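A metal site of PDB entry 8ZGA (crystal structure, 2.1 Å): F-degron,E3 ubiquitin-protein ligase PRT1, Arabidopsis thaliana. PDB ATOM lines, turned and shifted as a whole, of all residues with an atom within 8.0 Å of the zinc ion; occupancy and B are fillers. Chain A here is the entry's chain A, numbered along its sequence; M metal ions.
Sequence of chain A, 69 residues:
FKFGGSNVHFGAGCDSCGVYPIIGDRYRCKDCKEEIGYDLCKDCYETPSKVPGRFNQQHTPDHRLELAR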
ATOM      1  N   ARG A  28      -5.907 -15.796 -23.742  1.00  0.00           N
ATOM      2  CA  ARG A  28      -4.766 -15.189 -23.080  1.00  0.00           C
ATOM      3  C   ARG A  28      -3.865 -14.533 -24.112  1.00  0.00           C
ATOM      4  O   ARG A  28      -3.820 -14.964 -25.277  1.00  0.00           O
ATOM      5  CB  ARG A  28      -4.001 -16.266 -22.298  1.00  0.00           C
ATOM      6  CG  ARG A  28      -2.609 -15.891 -21.853  1.00  0.00           C
ATOM      7  CD  ARG A  28      -2.015 -17.001 -21.013  1.00  0.00           C
ATOM      8  NE  ARG A  28      -0.597 -17.189 -21.264  1.00  0.00           N
ATOM      9  CZ  ARG A  28       0.357 -16.486 -20.668  1.00  0.00           C
ATOM     10  NH1 ARG A  28       1.639 -16.727 -20.944  1.00  0.00           N
ATOM     11  NH2 ARG A  28       0.032 -15.562 -19.785  1.00  0.00           N
ATOM     12  N   CYS A  29      -3.129 -13.509 -23.691  1.00  0.00           N
ATOM     13  CA  CYS A  29      -2.251 -12.770 -24.570  1.00  0.00           C
ATOM     14  C   CYS A  29      -0.877 -13.408 -24.569  1.00  0.00           C
ATOM     15  O   CYS A  29      -0.360 -13.794 -23.526  1.00  0.00           O
ATOM     16  CB  CYS A  29      -2.137 -11.317 -24.121  1.00  0.00           C
ATOM     17  SG  CYS A  29      -1.108 -10.308 -25.235  1.00  0.00           S
ATOM     18  N   LYS A  30      -0.297 -13.526 -25.760  1.00  0.00           N
ATOM     19  CA  LYS A  30       1.050 -14.052 -25.914  1.00  0.00           C
ATOM     20  C   LYS A  30       2.133 -12.983 -25.790  1.00  0.00           C
ATOM     21  O   LYS A  30       3.274 -13.311 -25.423  1.00  0.00           O
ATOM     22  CB  LYS A  30       1.218 -14.739 -27.269  1.00  0.00           C
ATOM     23  CG  LYS A  30       0.305 -15.911 -27.543  1.00  0.00           C
ATOM     24  CD  LYS A  30       0.673 -16.533 -28.898  1.00  0.00           C
ATOM     25  CE  LYS A  30      -0.194 -17.724 -29.259  1.00  0.00           C
ATOM     26  NZ  LYS A  30       0.254 -18.271 -30.569  1.00  0.00           N
ATOM     27  N   ASP A  31       1.794 -11.725 -26.077  1.00  0.00           N
ATOM     28  CA  ASP A  31       2.793 -10.661 -26.148  1.00  0.00           C
ATOM     29  C   ASP A  31       2.847  -9.798 -24.900  1.00  0.00           C
ATOM     30  O   ASP A  31       3.892  -9.220 -24.600  1.00  0.00           O
ATOM     31  CB  ASP A  31       2.502  -9.773 -27.371  1.00  0.00           C
ATOM     32  CG  ASP A  31       2.266 -10.592 -28.632  1.00  0.00           C
ATOM     33  OD1 ASP A  31       3.016 -11.562 -28.879  1.00  0.00           O
ATOM     34  OD2 ASP A  31       1.309 -10.271 -29.374  1.00  0.00           O
ATOM     35  N   CYS A  32       1.744  -9.694 -24.158  1.00  0.00           N
ATOM     36  CA  CYS A  32       1.774  -9.021 -22.872  1.00  0.00           C
ATOM     37  C   CYS A  32       2.610  -9.828 -21.890  1.00  0.00           C
ATOM     38  O   CYS A  32       2.216 -10.938 -21.504  1.00  0.00           O
ATOM     39  CB  CYS A  32       0.355  -8.814 -22.333  1.00  0.00           C
ATOM     40  SG  CYS A  32      -0.548  -7.420 -23.076  1.00  0.00           S
ATOM     41  N   LYS A  33       3.755  -9.285 -21.473  1.00  0.00           N
ATOM     42  CA  LYS A  33       4.658  -9.988 -20.582  1.00  0.00           C
ATOM     43  C   LYS A  33       4.495  -9.575 -19.127  1.00  0.00           C
ATOM     44  O   LYS A  33       5.232 -10.086 -18.274  1.00  0.00           O
ATOM     45  CB  LYS A  33       6.124  -9.771 -21.003  1.00  0.00           C
ATOM     46  CG  LYS A  33       6.353  -9.840 -22.501  1.00  0.00           C
ATOM     47  CD  LYS A  33       5.938 -11.177 -23.077  1.00  0.00           C
ATOM     48  CE  LYS A  33       6.286 -11.220 -24.537  1.00  0.00           C
ATOM     49  NZ  LYS A  33       5.727 -12.395 -25.212  1.00  0.00           N
ATOM     50  N   GLU A  34       3.564  -8.673 -18.816  1.00  0.00           N
ATOM     51  CA  GLU A  34       3.273  -8.373 -17.425  1.00  0.00           C
ATOM     52  C   GLU A  34       2.907  -9.658 -16.682  1.00  0.00           C
ATOM     53  O   GLU A  34       2.182 -10.512 -17.210  1.00  0.00           O
ATOM     54  CB  GLU A  34       2.143  -7.347 -17.317  1.00  0.00           C
ATOM     55  CG  GLU A  34       2.461  -5.993 -17.955  1.00  0.00           C
ATOM     56  CD  GLU A  34       2.241  -5.987 -19.451  1.00  0.00           C
ATOM     57  OE1 GLU A  34       1.962  -7.070 -20.013  1.00  0.00           O
ATOM     58  OE2 GLU A  34       2.318  -4.899 -20.066  1.00  0.00           O
ATOM     59  N   GLY A  37      -0.512 -10.579 -16.597  1.00  0.00           N
ATOM     60  CA  GLY A  37      -1.001 -11.112 -17.849  1.00  0.00           C
ATOM     61  C   GLY A  37      -2.227 -10.376 -18.344  1.00  0.00           C
ATOM     62  O   GLY A  37      -2.691  -9.400 -17.761  1.00  0.00           O
ATOM     63  N   TYR A  38      -2.749 -10.854 -19.470  1.00  0.00           N
ATOM     64  CA  TYR A  38      -3.932 -10.271 -20.081  1.00  0.00           C
ATOM     65  C   TYR A  38      -4.857 -11.388 -20.560  1.00  0.00           C
ATOM     66  O   TYR A  38      -4.413 -12.289 -21.273  1.00  0.00           O
ATOM     67  CB  TYR A  38      -3.556  -9.365 -21.258  1.00  0.00           C
ATOM     68  CG  TYR A  38      -4.758  -8.703 -21.901  1.00  0.00           C
ATOM     69  CD1 TYR A  38      -5.467  -9.333 -22.915  1.00  0.00           C
ATOM     70  CD2 TYR A  38      -5.183  -7.453 -21.479  1.00  0.00           C
ATOM     71  CE1 TYR A  38      -6.557  -8.736 -23.498  1.00  0.00           C
ATOM     72  CE2 TYR A  38      -6.281  -6.848 -22.055  1.00  0.00           C
ATOM     73  CZ  TYR A  38      -6.956  -7.488 -23.061  1.00  0.00           C
ATOM     74  OH  TYR A  38      -8.055  -6.891 -23.642  1.00  0.00           O
ATOM     75  N   ASP A  39      -6.126 -11.306 -20.165  1.00  0.00           N
ATOM     76  CA  ASP A  39      -7.094 -12.348 -20.490  1.00  0.00           C
ATOM     77  C   ASP A  39      -8.428 -11.717 -20.856  1.00  0.00           C
ATOM     78  O   ASP A  39      -8.749 -10.605 -20.429  1.00  0.00           O
ATOM     79  CB  ASP A  39      -7.285 -13.319 -19.323  1.00  0.00           C
ATOM     80  CG  ASP A  39      -5.978 -13.952 -18.877  1.00  0.00           C
ATOM     81  OD1 ASP A  39      -5.215 -13.293 -18.152  1.00  0.00           O
ATOM     82  OD2 ASP A  39      -5.730 -15.117 -19.266  1.00  0.00           O
ATOM     83  N   VAL A  51      -9.857  -2.653 -25.081  1.00  0.00           N
ATOM     84  CA  VAL A  51      -9.633  -3.102 -23.707  1.00  0.00           C
ATOM     85  C   VAL A  51      -8.119  -3.018 -23.450  1.00  0.00           C
ATOM     86  O   VAL A  51      -7.397  -4.000 -23.622  1.00  0.00           O
ATOM     87  CB  VAL A  51     -10.190  -4.521 -23.479  1.00  0.00           C
ATOM     88  CG1 VAL A  51     -10.027  -4.963 -22.033  1.00  0.00           C
ATOM     89  CG2 VAL A  51     -11.676  -4.604 -23.877  1.00  0.00           C
ATOM     90  N   PRO A  52      -7.622  -1.842 -23.032  1.00  0.00           N
ATOM     91  CA  PRO A  52      -6.209  -1.770 -22.631  1.00  0.00           C
ATOM     92  C   PRO A  52      -5.894  -2.679 -21.463  1.00  0.00           C
ATOM     93  O   PRO A  52      -4.747  -3.135 -21.332  1.00  0.00           O
ATOM     94  CB  PRO A  52      -6.030  -0.285 -22.243  1.00  0.00           C
ATOM     95  CG  PRO A  52      -7.397   0.218 -21.953  1.00  0.00           C
ATOM     96  CD  PRO A  52      -8.340  -0.575 -22.835  1.00  0.00           C
ATOM     97  N   GLN A  57      -1.898  -3.129 -18.074  1.00  0.00           N
ATOM     98  CA  GLN A  57      -1.394  -3.915 -19.195  1.00  0.00           C
ATOM     99  C   GLN A  57      -1.324  -3.030 -20.436  1.00  0.00           C
ATOM    100  O   GLN A  57      -2.286  -2.321 -20.763  1.00  0.00           O
ATOM    101  CB  GLN A  57      -2.303  -5.119 -19.454  1.00  0.00           C
ATOM    102  CG  GLN A  57      -2.488  -6.041 -18.273  1.00  0.00           C
ATOM    103  CD  GLN A  57      -3.822  -5.831 -17.601  1.00  0.00           C
ATOM    104  OE1 GLN A  57      -4.199  -4.713 -17.249  1.00  0.00           O
ATOM    105  NE2 GLN A  57      -4.566  -6.923 -17.421  1.00  0.00           N
ATOM    106  N   GLN A  58      -0.192  -3.076 -21.128  1.00  0.00           N
ATOM    107  CA  GLN A  58       0.005  -2.313 -22.360  1.00  0.00           C
ATOM    108  C   GLN A  58      -0.443  -3.158 -23.560  1.00  0.00           C
ATOM    109  O   GLN A  58       0.338  -3.518 -24.439  1.00  0.00           O
ATOM    110  CB  GLN A  58       1.467  -1.886 -22.485  1.00  0.00           C
ATOM    111  CG  GLN A  58       1.994  -1.097 -21.295  1.00  0.00           C
ATOM    112  CD  GLN A  58       1.527   0.344 -21.277  1.00  0.00           C
ATOM    113  OE1 GLN A  58       1.086   0.883 -22.289  1.00  0.00           O
ATOM    114  NE2 GLN A  58       1.624   0.976 -20.108  1.00  0.00           N
ATOM    115  N   HIS A  59      -1.732  -3.482 -23.559  1.00  0.00           N
ATOM    116  CA  HIS A  59      -2.311  -4.354 -24.577  1.00  0.00           C
ATOM    117  C   HIS A  59      -2.741  -3.511 -25.773  1.00  0.00           C
ATOM    118  O   HIS A  59      -3.539  -2.588 -25.636  1.00  0.00           O
ATOM    119  CB  HIS A  59      -3.499  -5.121 -24.005  1.00  0.00           C
ATOM    120  CG  HIS A  59      -4.079  -6.135 -24.951  1.00  0.00           C
ATOM    121  ND1 HIS A  59      -3.505  -7.359 -25.175  1.00  0.00           N
ATOM    122  CD2 HIS A  59      -5.182  -6.084 -25.737  1.00  0.00           C
ATOM    123  CE1 HIS A  59      -4.225  -8.035 -26.056  1.00  0.00           C
ATOM    124  NE2 HIS A  59      -5.249  -7.272 -26.416  1.00  0.00           N
ATOM    125  N   THR A  60      -2.202  -3.839 -26.944  1.00  0.00           N
ATOM    126  CA  THR A  60      -2.502  -3.161 -28.181  1.00  0.00           C
ATOM    127  C   THR A  60      -3.302  -4.078 -29.098  1.00  0.00           C
ATOM    128  O   THR A  60      -3.254  -5.300 -28.964  1.00  0.00           O
ATOM    129  CB  THR A  60      -1.213  -2.735 -28.905  1.00  0.00           C
ATOM    130  OG1 THR A  60      -0.533  -3.898 -29.390  1.00  0.00           O
ATOM    131  CG2 THR A  60      -0.302  -1.971 -27.958  1.00  0.00           C
ATOM    132  N   PRO A  61      -4.067  -3.512 -30.042  1.00  0.00           N
ATOM    133  CA  PRO A  61      -4.794  -4.377 -30.998  1.00  0.00           C
ATOM    134  C   PRO A  61      -3.885  -5.329 -31.765  1.00  0.00           C
ATOM    135  O   PRO A  61      -4.361  -6.354 -32.256  1.00  0.00           O
ATOM    136  CB  PRO A  61      -5.467  -3.367 -31.945  1.00  0.00           C
ATOM    137  CG  PRO A  61      -5.598  -2.119 -31.133  1.00  0.00           C
ATOM    138  CD  PRO A  61      -4.388  -2.085 -30.222  1.00  0.00           C
ATOM    139  N   ASP A  62      -2.586  -5.023 -31.863  1.00  0.00           N
ATOM    140  CA  ASP A  62      -1.649  -5.921 -32.547  1.00  0.00           C
ATOM    141  C   ASP A  62      -1.339  -7.172 -31.728  1.00  0.00           C
ATOM    142  O   ASP A  62      -0.906  -8.178 -32.307  1.00  0.00           O
ATOM    143  CB  ASP A  62      -0.350  -5.184 -32.869  1.00  0.00           C
ATOM    144  CG  ASP A  62      -0.573  -3.886 -33.615  1.00  0.00           C
ATOM    145  OD1 ASP A  62      -0.928  -2.878 -32.962  1.00  0.00           O
ATOM    146  OD2 ASP A  62      -0.403  -3.866 -34.850  1.00  0.00           O
ATOM    147  N   HIS A  63      -1.534  -7.137 -30.416  1.00  0.00           N
ATOM    148  CA  HIS A  63      -1.308  -8.321 -29.603  1.00  0.00           C
ATOM    149  C   HIS A  63      -2.226  -9.453 -30.057  1.00  0.00           C
ATOM    150  O   HIS A  63      -3.369  -9.236 -30.453  1.00  0.00           O
ATOM    151  CB  HIS A  63      -1.542  -8.005 -28.135  1.00  0.00           C
ATOM    152  CG  HIS A  63      -0.450  -7.197 -27.508  1.00  0.00           C
ATOM    153  ND1 HIS A  63      -0.251  -7.175 -26.144  1.00  0.00           N
ATOM    154  CD2 HIS A  63       0.471  -6.369 -28.032  1.00  0.00           C
ATOM    155  CE1 HIS A  63       0.773  -6.388 -25.858  1.00  0.00           C
ATOM    156  NE2 HIS A  63       1.228  -5.890 -26.991  1.00  0.00           N
ATOM    157  N   ARG A  64      -1.723 -10.690 -29.976  1.00  0.00           N
ATOM    158  CA  ARG A  64      -2.467 -11.871 -30.380  1.00  0.00           C
ATOM    159  C   ARG A  64      -2.885 -12.648 -29.148  1.00  0.00           C
ATOM    160  O   ARG A  64      -2.145 -12.718 -28.153  1.00  0.00           O
ATOM    161  CB  ARG A  64      -1.615 -12.756 -31.295  1.00  0.00           C
ATOM    162  CG  ARG A  64      -2.397 -13.724 -32.187  1.00  0.00           C
ATOM    163  CD  ARG A  64      -1.437 -14.547 -33.062  1.00  0.00           C
ATOM    164  NE  ARG A  64      -0.314 -13.716 -33.515  1.00  0.00           N
ATOM    165  CZ  ARG A  64       0.851 -13.633 -32.873  1.00  0.00           C
ATOM    166  NH1 ARG A  64       1.058 -14.329 -31.762  1.00  0.00           N
ATOM    167  NH2 ARG A  64       1.812 -12.845 -33.338  1.00  0.00           N
ATOM    168  N   LEU A  65      -4.090 -13.228 -29.195  1.00  0.00           N
ATOM    169  CA  LEU A  65      -4.649 -13.964 -28.076  1.00  0.00           C
ATOM    170  C   LEU A  65      -4.879 -15.409 -28.496  1.00  0.00           C
ATOM    171  O   LEU A  65      -5.357 -15.667 -29.600  1.00  0.00           O
ATOM    172  CB  LEU A  65      -5.958 -13.352 -27.581  1.00  0.00           C
ATOM    173  CG  LEU A  65      -5.854 -11.892 -27.162  1.00  0.00           C
ATOM    174  CD1 LEU A  65      -7.202 -11.330 -26.817  1.00  0.00           C
ATOM    175  CD2 LEU A  65      -4.929 -11.766 -25.998  1.00  0.00           C
HETATM  176 ZN    ZN M   1      -1.619  -8.081 -24.949  1.00  0.00          ZN
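N of Cys 29 is in hydrogen-bond range of O of Tyr 38 (3.0 Å). The side-chain sulfur (SG) of Cys 29 lies close to the backbone NH (N) of Asp 31 (3.3 Å).
Of the 21 residues printed, 4 come within 4 Å of the zinc ion. The nearest printed residue that does not touch the zinc ion is Tyr 38 (4.4 Å).
The zinc ion is bound by ND1 of His 63 (2.0 Å). A ring nitrogen (ND1) of His 59 is bound to the zinc ion, at 2.0 Å. The zinc ion is bound by the side-chain sulfur (SG) of Cys 32, 2.3 Å away. SG of Cys 29 binds the zinc ion. The zinc ion has four donor atoms within binding distance.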
